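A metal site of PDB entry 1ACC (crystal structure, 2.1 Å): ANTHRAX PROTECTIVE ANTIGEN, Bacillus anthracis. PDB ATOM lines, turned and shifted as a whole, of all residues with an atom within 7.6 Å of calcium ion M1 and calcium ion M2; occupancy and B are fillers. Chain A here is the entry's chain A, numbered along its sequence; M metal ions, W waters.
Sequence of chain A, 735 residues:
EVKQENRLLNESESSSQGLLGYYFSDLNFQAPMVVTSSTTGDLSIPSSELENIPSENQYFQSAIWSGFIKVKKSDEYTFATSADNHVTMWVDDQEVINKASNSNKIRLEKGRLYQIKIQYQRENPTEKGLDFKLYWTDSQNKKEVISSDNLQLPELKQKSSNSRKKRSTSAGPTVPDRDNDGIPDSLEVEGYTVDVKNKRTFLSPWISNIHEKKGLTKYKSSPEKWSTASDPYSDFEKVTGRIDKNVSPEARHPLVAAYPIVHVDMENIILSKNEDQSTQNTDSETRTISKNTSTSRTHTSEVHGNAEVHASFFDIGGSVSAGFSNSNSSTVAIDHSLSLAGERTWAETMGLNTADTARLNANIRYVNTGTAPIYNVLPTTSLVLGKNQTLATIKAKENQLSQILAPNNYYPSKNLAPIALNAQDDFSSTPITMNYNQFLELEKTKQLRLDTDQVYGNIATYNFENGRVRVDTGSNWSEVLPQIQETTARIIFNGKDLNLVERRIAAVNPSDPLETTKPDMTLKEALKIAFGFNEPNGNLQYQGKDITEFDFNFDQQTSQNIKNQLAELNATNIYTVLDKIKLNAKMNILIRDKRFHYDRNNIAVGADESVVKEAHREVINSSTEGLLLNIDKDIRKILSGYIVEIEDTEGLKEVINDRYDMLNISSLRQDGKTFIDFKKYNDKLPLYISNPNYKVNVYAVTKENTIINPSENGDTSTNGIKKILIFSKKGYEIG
Within 4 Å of calcium ion M1: Asp 177, Asp 179, Asp 181, Ile 183 and Glu 188.
The backbone NH (N) of Lys 225 is in hydrogen-bond range of the side-chain hydroxyl (OG) of Ser 222, 3.3 Å away. The side-chain hydroxyl (OG1) of Thr 228 sits at hydrogen-bond distance from the backbone NH (N) of Ser 222 (2.8 Å). The backbone NH (N) of Glu 224 lies close to the side-chain hydroxyl (OG) of Ser 222 (3.1 Å). The side-chain carboxylate (OD1) of Asp 235 is in hydrogen-bond range of the backbone NH (N) of Thr 228 (2.9 Å). The backbone NH (N) of Asp 235 lies within hydrogen-bond range of the backbone carbonyl oxygen (O) of Trp 226 (3.1 Å). The side-chain carboxylate (OD2) of Asp 177 sits at hydrogen-bond distance from the backbone NH (N) of Gly 182 (2.7 Å). OD1 of Asp 177 lies close to N of Asn 180 (3.3 Å). The side-chain amino group of Lys 225 sits at hydrogen-bond distance from the backbone carbonyl oxygen of Thr 228.
Calcium ion M2 is bound by O of Ser 222, OD2 of Asp 179, OD2 of Asp 235, OE1 of Glu 188, OD2 of Asp 181 and O of Lys 225. Slightly farther from calcium ion M2 lies the side-chain carboxylate (OE2) of Glu 188 (3.0 Å).
Calcium ion M1 is bound by water W1. OD1 of Asp 177 is bound to calcium ion M1, 2.3 Å away. OD1 of Asp 181 binds calcium ion M1. Calcium ion M1 is bound by O of Ile 183 (2.4 Å). Calcium ion M1 is bound by OE2 of Glu 188, 2.4 Å away. Calcium ion M1 is bound by OD1 of Asp 179, at 2.4 Å.
Within 4 Å of calcium ion M2: Asp 179, Asp 181, Glu 188, Ser 222, Lys 225 and Asp 235. The nearest printed residue that does not touch calcium ion M2 is Thr 228 (4.01 Å).
Water W1 lies within hydrogen-bond range of the side-chain carboxylate (OD1) of Asp 185 (2.7 Å), the backbone carbonyl oxygen (O) of Pro 223 (3.0 Å), the backbone NH (N) of Arg 178 (3.4 Å) and the backbone NH (N) of Asp 179 (3.5 Å).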
ATOM      1  N   TYR A  22      16.830  -8.731 -11.447  1.00  0.00           N
ATOM      2  CA  TYR A  22      15.588  -9.422 -11.734  1.00  0.00           C
ATOM      3  C   TYR A  22      15.522  -9.493 -13.254  1.00  0.00           C
ATOM      4  O   TYR A  22      15.592  -8.462 -13.925  1.00  0.00           O
ATOM      5  CB  TYR A  22      14.399  -8.615 -11.199  1.00  0.00           C
ATOM      6  CG  TYR A  22      14.385  -8.487  -9.694  1.00  0.00           C
ATOM      7  CD1 TYR A  22      15.134  -7.511  -9.053  1.00  0.00           C
ATOM      8  CD2 TYR A  22      13.620  -9.358  -8.912  1.00  0.00           C
ATOM      9  CE1 TYR A  22      15.142  -7.409  -7.667  1.00  0.00           C
ATOM     10  CE2 TYR A  22      13.614  -9.260  -7.526  1.00  0.00           C
ATOM     11  CZ  TYR A  22      14.379  -8.286  -6.909  1.00  0.00           C
ATOM     12  OH  TYR A  22      14.378  -8.210  -5.542  1.00  0.00           O
ATOM     13  N   PRO A 176       7.938  -5.461  -7.170  1.00  0.00           N
ATOM     14  CA  PRO A 176       6.868  -5.712  -6.195  1.00  0.00           C
ATOM     15  C   PRO A 176       7.395  -6.658  -5.148  1.00  0.00           C
ATOM     16  O   PRO A 176       7.524  -7.866  -5.386  1.00  0.00           O
ATOM     17  CB  PRO A 176       5.776  -6.389  -7.036  1.00  0.00           C
ATOM     18  CG  PRO A 176       6.233  -6.245  -8.479  1.00  0.00           C
ATOM     19  CD  PRO A 176       7.721  -6.289  -8.370  1.00  0.00           C
ATOM     20  N   ASP A 177       7.694  -6.108  -3.985  1.00  0.00           N
ATOM     21  CA  ASP A 177       8.245  -6.889  -2.889  1.00  0.00           C
ATOM     22  C   ASP A 177       7.762  -6.207  -1.618  1.00  0.00           C
ATOM     23  O   ASP A 177       8.494  -5.455  -0.973  1.00  0.00           O
ATOM     24  CB  ASP A 177       9.768  -6.832  -3.013  1.00  0.00           C
ATOM     25  CG  ASP A 177      10.486  -7.636  -1.952  1.00  0.00           C
ATOM     26  OD1 ASP A 177       9.844  -8.383  -1.189  1.00  0.00           O
ATOM     27  OD2 ASP A 177      11.715  -7.484  -1.887  1.00  0.00           O
ATOM     28  N   ARG A 178       6.489  -6.424  -1.308  1.00  0.00           N
ATOM     29  CA  ARG A 178       5.849  -5.843  -0.135  1.00  0.00           C
ATOM     30  C   ARG A 178       6.611  -5.939   1.176  1.00  0.00           C
ATOM     31  O   ARG A 178       6.574  -4.992   1.972  1.00  0.00           O
ATOM     32  CB  ARG A 178       4.441  -6.427   0.051  1.00  0.00           C
ATOM     33  CG  ARG A 178       3.436  -6.026  -1.018  1.00  0.00           C
ATOM     34  CD  ARG A 178       2.041  -6.577  -0.725  1.00  0.00           C
ATOM     35  NE  ARG A 178       1.960  -8.029  -0.852  1.00  0.00           N
ATOM     36  CZ  ARG A 178       1.134  -8.662  -1.680  1.00  0.00           C
ATOM     37  NH1 ARG A 178       0.298  -7.974  -2.441  1.00  0.00           N
ATOM     38  NH2 ARG A 178       1.132  -9.989  -1.736  1.00  0.00           N
ATOM     39  N   ASP A 179       7.292  -7.057   1.427  1.00  0.00           N
ATOM     40  CA  ASP A 179       8.021  -7.225   2.681  1.00  0.00           C
ATOM     41  C   ASP A 179       9.517  -6.943   2.643  1.00  0.00           C
ATOM     42  O   ASP A 179      10.227  -7.150   3.628  1.00  0.00           O
ATOM     43  CB  ASP A 179       7.754  -8.611   3.280  1.00  0.00           C
ATOM     44  CG  ASP A 179       8.143  -9.743   2.342  1.00  0.00           C
ATOM     45  OD1 ASP A 179       8.830  -9.507   1.341  1.00  0.00           O
ATOM     46  OD2 ASP A 179       7.738 -10.890   2.624  1.00  0.00           O
ATOM     47  N   ASN A 180      10.017  -6.532   1.478  1.00  0.00           N
ATOM     48  CA  ASN A 180      11.430  -6.206   1.314  1.00  0.00           C
ATOM     49  C   ASN A 180      12.426  -7.335   1.576  1.00  0.00           C
ATOM     50  O   ASN A 180      13.565  -7.084   1.944  1.00  0.00           O
ATOM     51  CB  ASN A 180      11.777  -4.987   2.177  1.00  0.00           C
ATOM     52  CG  ASN A 180      13.099  -4.344   1.786  1.00  0.00           C
ATOM     53  OD1 ASN A 180      13.956  -4.109   2.633  1.00  0.00           O
ATOM     54  ND2 ASN A 180      13.242  -4.024   0.511  1.00  0.00           N
ATOM     55  N   ASP A 181      12.004  -8.584   1.394  1.00  0.00           N
ATOM     56  CA  ASP A 181      12.944  -9.691   1.583  1.00  0.00           C
ATOM     57  C   ASP A 181      13.723  -9.943   0.296  1.00  0.00           C
ATOM     58  O   ASP A 181      14.787 -10.544   0.309  1.00  0.00           O
ATOM     59  CB  ASP A 181      12.273 -10.972   2.139  1.00  0.00           C
ATOM     60  CG  ASP A 181      11.148 -11.511   1.245  1.00  0.00           C
ATOM     61  OD1 ASP A 181      11.091 -11.204   0.036  1.00  0.00           O
ATOM     62  OD2 ASP A 181      10.314 -12.273   1.784  1.00  0.00           O
ATOM     63  N   GLY A 182      13.188  -9.439  -0.819  1.00  0.00           N
ATOM     64  CA  GLY A 182      13.865  -9.603  -2.096  1.00  0.00           C
ATOM     65  C   GLY A 182      13.148 -10.468  -3.116  1.00  0.00           C
ATOM     66  O   GLY A 182      13.421 -10.383  -4.308  1.00  0.00           O
ATOM     67  N   ILE A 183      12.279 -11.356  -2.653  1.00  0.00           N
ATOM     68  CA  ILE A 183      11.551 -12.237  -3.560  1.00  0.00           C
ATOM     69  C   ILE A 183      10.258 -11.533  -3.975  1.00  0.00           C
ATOM     70  O   ILE A 183       9.518 -11.044  -3.128  1.00  0.00           O
ATOM     71  CB  ILE A 183      11.164 -13.583  -2.882  1.00  0.00           C
ATOM     72  CG1 ILE A 183      12.351 -14.158  -2.109  1.00  0.00           C
ATOM     73  CG2 ILE A 183      10.684 -14.582  -3.929  1.00  0.00           C
ATOM     74  CD1 ILE A 183      12.006 -15.344  -1.235  1.00  0.00           C
ATOM     75  N   PRO A 184       9.995 -11.452  -5.293  1.00  0.00           N
ATOM     76  CA  PRO A 184       8.776 -10.809  -5.823  1.00  0.00           C
ATOM     77  C   PRO A 184       7.544 -11.434  -5.166  1.00  0.00           C
ATOM     78  O   PRO A 184       7.532 -12.636  -4.895  1.00  0.00           O
ATOM     79  CB  PRO A 184       8.842 -11.151  -7.306  1.00  0.00           C
ATOM     80  CG  PRO A 184      10.296 -11.138  -7.580  1.00  0.00           C
ATOM     81  CD  PRO A 184      10.863 -11.893  -6.401  1.00  0.00           C
ATOM     82  N   ASP A 185       6.513 -10.615  -4.919  1.00  0.00           N
ATOM     83  CA  ASP A 185       5.291 -11.103  -4.286  1.00  0.00           C
ATOM     84  C   ASP A 185       4.693 -12.279  -5.036  1.00  0.00           C
ATOM     85  O   ASP A 185       4.188 -13.226  -4.434  1.00  0.00           O
ATOM     86  CB  ASP A 185       4.221 -10.000  -4.230  1.00  0.00           C
ATOM     87  CG  ASP A 185       4.709  -8.731  -3.585  1.00  0.00           C
ATOM     88  OD1 ASP A 185       5.632  -8.795  -2.748  1.00  0.00           O
ATOM     89  OD2 ASP A 185       4.152  -7.671  -3.911  1.00  0.00           O
ATOM     90  N   SER A 186       4.658 -12.149  -6.355  1.00  0.00           N
ATOM     91  CA  SER A 186       4.109 -13.170  -7.234  1.00  0.00           C
ATOM     92  C   SER A 186       4.755 -14.534  -7.029  1.00  0.00           C
ATOM     93  O   SER A 186       4.064 -15.547  -6.928  1.00  0.00           O
ATOM     94  CB  SER A 186       4.239 -12.731  -8.699  1.00  0.00           C
ATOM     95  OG  SER A 186       5.553 -12.295  -9.005  1.00  0.00           O
ATOM     96  N   GLU A 188       6.510 -15.667  -4.372  1.00  0.00           N
ATOM     97  CA  GLU A 188       6.265 -16.199  -3.039  1.00  0.00           C
ATOM     98  C   GLU A 188       4.897 -16.885  -3.002  1.00  0.00           C
ATOM     99  O   GLU A 188       4.761 -18.002  -2.508  1.00  0.00           O
ATOM    100  CB  GLU A 188       6.347 -15.088  -1.989  1.00  0.00           C
ATOM    101  CG  GLU A 188       7.761 -14.562  -1.768  1.00  0.00           C
ATOM    102  CD  GLU A 188       7.927 -13.826  -0.448  1.00  0.00           C
ATOM    103  OE1 GLU A 188       8.101 -14.492   0.595  1.00  0.00           O
ATOM    104  OE2 GLU A 188       7.877 -12.582  -0.450  1.00  0.00           O
ATOM    105  N   TYR A 192       8.304 -20.900  -5.958  1.00  0.00           N
ATOM    106  CA  TYR A 192       9.604 -20.612  -6.512  1.00  0.00           C
ATOM    107  C   TYR A 192      10.584 -21.678  -6.065  1.00  0.00           C
ATOM    108  O   TYR A 192      10.250 -22.551  -5.268  1.00  0.00           O
ATOM    109  CB  TYR A 192      10.079 -19.228  -6.048  1.00  0.00           C
ATOM    110  CG  TYR A 192      10.173 -19.060  -4.537  1.00  0.00           C
ATOM    111  CD1 TYR A 192       9.053 -18.689  -3.786  1.00  0.00           C
ATOM    112  CD2 TYR A 192      11.380 -19.243  -3.877  1.00  0.00           C
ATOM    113  CE1 TYR A 192       9.150 -18.506  -2.409  1.00  0.00           C
ATOM    114  CE2 TYR A 192      11.486 -19.065  -2.503  1.00  0.00           C
ATOM    115  CZ  TYR A 192      10.373 -18.691  -1.772  1.00  0.00           C
ATOM    116  OH  TYR A 192      10.507 -18.513  -0.422  1.00  0.00           O
ATOM    117  N   SER A 221       6.133 -18.821   0.182  1.00  0.00           N
ATOM    118  CA  SER A 221       6.276 -18.050   1.400  1.00  0.00           C
ATOM    119  C   SER A 221       5.295 -16.896   1.382  1.00  0.00           C
ATOM    120  O   SER A 221       4.536 -16.729   0.429  1.00  0.00           O
ATOM    121  CB  SER A 221       7.717 -17.545   1.514  1.00  0.00           C
ATOM    122  OG  SER A 221       8.233 -17.138   0.250  1.00  0.00           O
ATOM    123  N   SER A 222       5.233 -16.179   2.490  1.00  0.00           N
ATOM    124  CA  SER A 222       4.330 -15.049   2.584  1.00  0.00           C
ATOM    125  C   SER A 222       4.982 -13.810   2.003  1.00  0.00           C
ATOM    126  O   SER A 222       6.114 -13.474   2.350  1.00  0.00           O
ATOM    127  CB  SER A 222       3.926 -14.782   4.026  1.00  0.00           C
ATOM    128  OG  SER A 222       3.165 -13.580   4.103  1.00  0.00           O
ATOM    129  N   PRO A 223       4.292 -13.150   1.068  1.00  0.00           N
ATOM    130  CA  PRO A 223       4.768 -11.935   0.419  1.00  0.00           C
ATOM    131  C   PRO A 223       4.576 -10.744   1.352  1.00  0.00           C
ATOM    132  O   PRO A 223       4.872  -9.601   0.992  1.00  0.00           O
ATOM    133  CB  PRO A 223       3.867 -11.837  -0.803  1.00  0.00           C
ATOM    134  CG  PRO A 223       2.570 -12.344  -0.267  1.00  0.00           C
ATOM    135  CD  PRO A 223       2.983 -13.566   0.515  1.00  0.00           C
ATOM    136  N   GLU A 224       4.010 -11.003   2.526  1.00  0.00           N
ATOM    137  CA  GLU A 224       3.761  -9.969   3.523  1.00  0.00           C
ATOM    138  C   GLU A 224       4.696 -10.112   4.704  1.00  0.00           C
ATOM    139  O   GLU A 224       4.742  -9.241   5.571  1.00  0.00           O
ATOM    140  CB  GLU A 224       2.332 -10.055   4.056  1.00  0.00           C
ATOM    141  CG  GLU A 224       1.281 -10.418   3.039  1.00  0.00           C
ATOM    142  CD  GLU A 224       0.964  -9.319   2.053  1.00  0.00           C
ATOM    143  OE1 GLU A 224       1.473  -8.189   2.194  1.00  0.00           O
ATOM    144  OE2 GLU A 224       0.176  -9.597   1.119  1.00  0.00           O
ATOM    145  N   LYS A 225       5.393 -11.238   4.790  1.00  0.00           N
ATOM    146  CA  LYS A 225       6.297 -11.465   5.911  1.00  0.00           C
ATOM    147  C   LYS A 225       7.747 -11.642   5.502  1.00  0.00           C
ATOM    148  O   LYS A 225       8.086 -12.573   4.772  1.00  0.00           O
ATOM    149  CB  LYS A 225       5.827 -12.647   6.754  1.00  0.00           C
ATOM    150  CG  LYS A 225       4.468 -12.424   7.417  1.00  0.00           C
ATOM    151  CD  LYS A 225       4.101 -13.586   8.334  1.00  0.00           C
ATOM    152  CE  LYS A 225       4.914 -13.559   9.621  1.00  0.00           C
ATOM    153  NZ  LYS A 225       4.784 -14.853  10.350  1.00  0.00           N
ATOM    154  N   TRP A 226       8.579 -10.705   5.939  1.00  0.00           N
ATOM    155  CA  TRP A 226      10.004 -10.723   5.667  1.00  0.00           C
ATOM    156  C   TRP A 226      10.542 -12.125   6.017  1.00  0.00           C
ATOM    157  O   TRP A 226      11.351 -12.683   5.288  1.00  0.00           O
ATOM    158  CB  TRP A 226      10.683  -9.610   6.450  1.00  0.00           C
ATOM    159  CG  TRP A 226      12.164  -9.532   6.306  1.00  0.00           C
ATOM    160  CD1 TRP A 226      12.872  -8.903   5.310  1.00  0.00           C
ATOM    161  CD2 TRP A 226      13.129 -10.065   7.210  1.00  0.00           C
ATOM    162  NE1 TRP A 226      14.217  -9.020   5.555  1.00  0.00           N
ATOM    163  CE2 TRP A 226      14.407  -9.719   6.712  1.00  0.00           C
ATOM    164  CE3 TRP A 226      13.044 -10.805   8.398  1.00  0.00           C
ATOM    165  CZ2 TRP A 226      15.588 -10.093   7.368  1.00  0.00           C
ATOM    166  CZ3 TRP A 226      14.217 -11.171   9.047  1.00  0.00           C
ATOM    167  CH2 TRP A 226      15.470 -10.812   8.524  1.00  0.00           C
ATOM    168  N   SER A 227      10.074 -12.665   7.132  1.00  0.00           N
ATOM    169  CA  SER A 227      10.427 -14.022   7.569  1.00  0.00           C
ATOM    170  C   SER A 227       9.069 -14.665   7.760  1.00  0.00           C
ATOM    171  O   SER A 227       8.269 -14.227   8.583  1.00  0.00           O
ATOM    172  CB  SER A 227      11.177 -14.008   8.911  1.00  0.00           C
ATOM    173  OG  SER A 227      11.486 -15.335   9.342  1.00  0.00           O
ATOM    174  N   THR A 228       8.736 -15.644   6.931  1.00  0.00           N
ATOM    175  CA  THR A 228       7.425 -16.266   7.040  1.00  0.00           C
ATOM    176  C   THR A 228       7.174 -17.012   8.358  1.00  0.00           C
ATOM    177  O   THR A 228       6.037 -17.042   8.812  1.00  0.00           O
ATOM    178  CB  THR A 228       7.082 -17.110   5.802  1.00  0.00           C
ATOM    179  OG1 THR A 228       7.060 -16.264   4.653  1.00  0.00           O
ATOM    180  CG2 THR A 228       5.686 -17.713   5.947  1.00  0.00           C
ATOM    181  N   SER A 234      15.347 -13.919   6.797  1.00  0.00           N
ATOM    182  CA  SER A 234      14.305 -13.783   5.784  1.00  0.00           C
ATOM    183  C   SER A 234      14.175 -14.970   4.838  1.00  0.00           C
ATOM    184  O   SER A 234      15.095 -15.782   4.722  1.00  0.00           O
ATOM    185  CB  SER A 234      14.478 -12.490   4.966  1.00  0.00           C
ATOM    186  OG  SER A 234      15.458 -12.614   3.954  1.00  0.00           O
ATOM    187  N   ASP A 235      13.049 -15.000   4.134  1.00  0.00           N
ATOM    188  CA  ASP A 235      12.751 -16.063   3.185  1.00  0.00           C
ATOM    189  C   ASP A 235      13.831 -16.148   2.116  1.00  0.00           C
ATOM    190  O   ASP A 235      14.242 -17.228   1.709  1.00  0.00           O
ATOM    191  CB  ASP A 235      11.379 -15.802   2.537  1.00  0.00           C
ATOM    192  CG  ASP A 235      10.248 -15.742   3.559  1.00  0.00           C
ATOM    193  OD1 ASP A 235      10.364 -16.378   4.629  1.00  0.00           O
ATOM    194  OD2 ASP A 235       9.242 -15.051   3.295  1.00  0.00           O
ATOM    195  N   PHE A 236      14.280 -14.975   1.657  1.00  0.00           N
ATOM    196  CA  PHE A 236      15.328 -14.873   0.649  1.00  0.00           C
ATOM    197  C   PHE A 236      16.692 -15.276   1.214  1.00  0.00           C
ATOM    198  O   PHE A 236      17.472 -15.956   0.538  1.00  0.00           O
ATOM    199  CB  PHE A 236      15.381 -13.445   0.085  1.00  0.00           C
ATOM    200  CG  PHE A 236      16.431 -13.231  -0.967  1.00  0.00           C
ATOM    201  CD1 PHE A 236      16.235 -13.666  -2.279  1.00  0.00           C
ATOM    202  CD2 PHE A 236      17.612 -12.559  -0.650  1.00  0.00           C
ATOM    203  CE1 PHE A 236      17.209 -13.439  -3.255  1.00  0.00           C
ATOM    204  CE2 PHE A 236      18.586 -12.332  -1.626  1.00  0.00           C
ATOM    205  CZ  PHE A 236      18.377 -12.774  -2.929  1.00  0.00           C
ATOM    206  N   PRO A 254      11.518 -21.599   4.292  1.00  0.00           N
ATOM    207  CA  PRO A 254      10.783 -20.444   4.820  1.00  0.00           C
ATOM    208  C   PRO A 254       9.530 -20.719   5.664  1.00  0.00           C
ATOM    209  O   PRO A 254       8.962 -19.803   6.249  1.00  0.00           O
ATOM    210  CB  PRO A 254      10.464 -19.631   3.567  1.00  0.00           C
ATOM    211  CG  PRO A 254      10.503 -20.641   2.458  1.00  0.00           C
ATOM    212  CD  PRO A 254      11.688 -21.474   2.835  1.00  0.00           C
HETATM  213 CA    CA M   1       9.034 -10.551  -0.866  1.00  0.00          CA
HETATM  214 CA    CA M   2       8.239 -13.112   2.479  1.00  0.00          CA
HETATM  215  O   HOH W   1       7.298  -9.707  -0.805  1.00  0.00           O
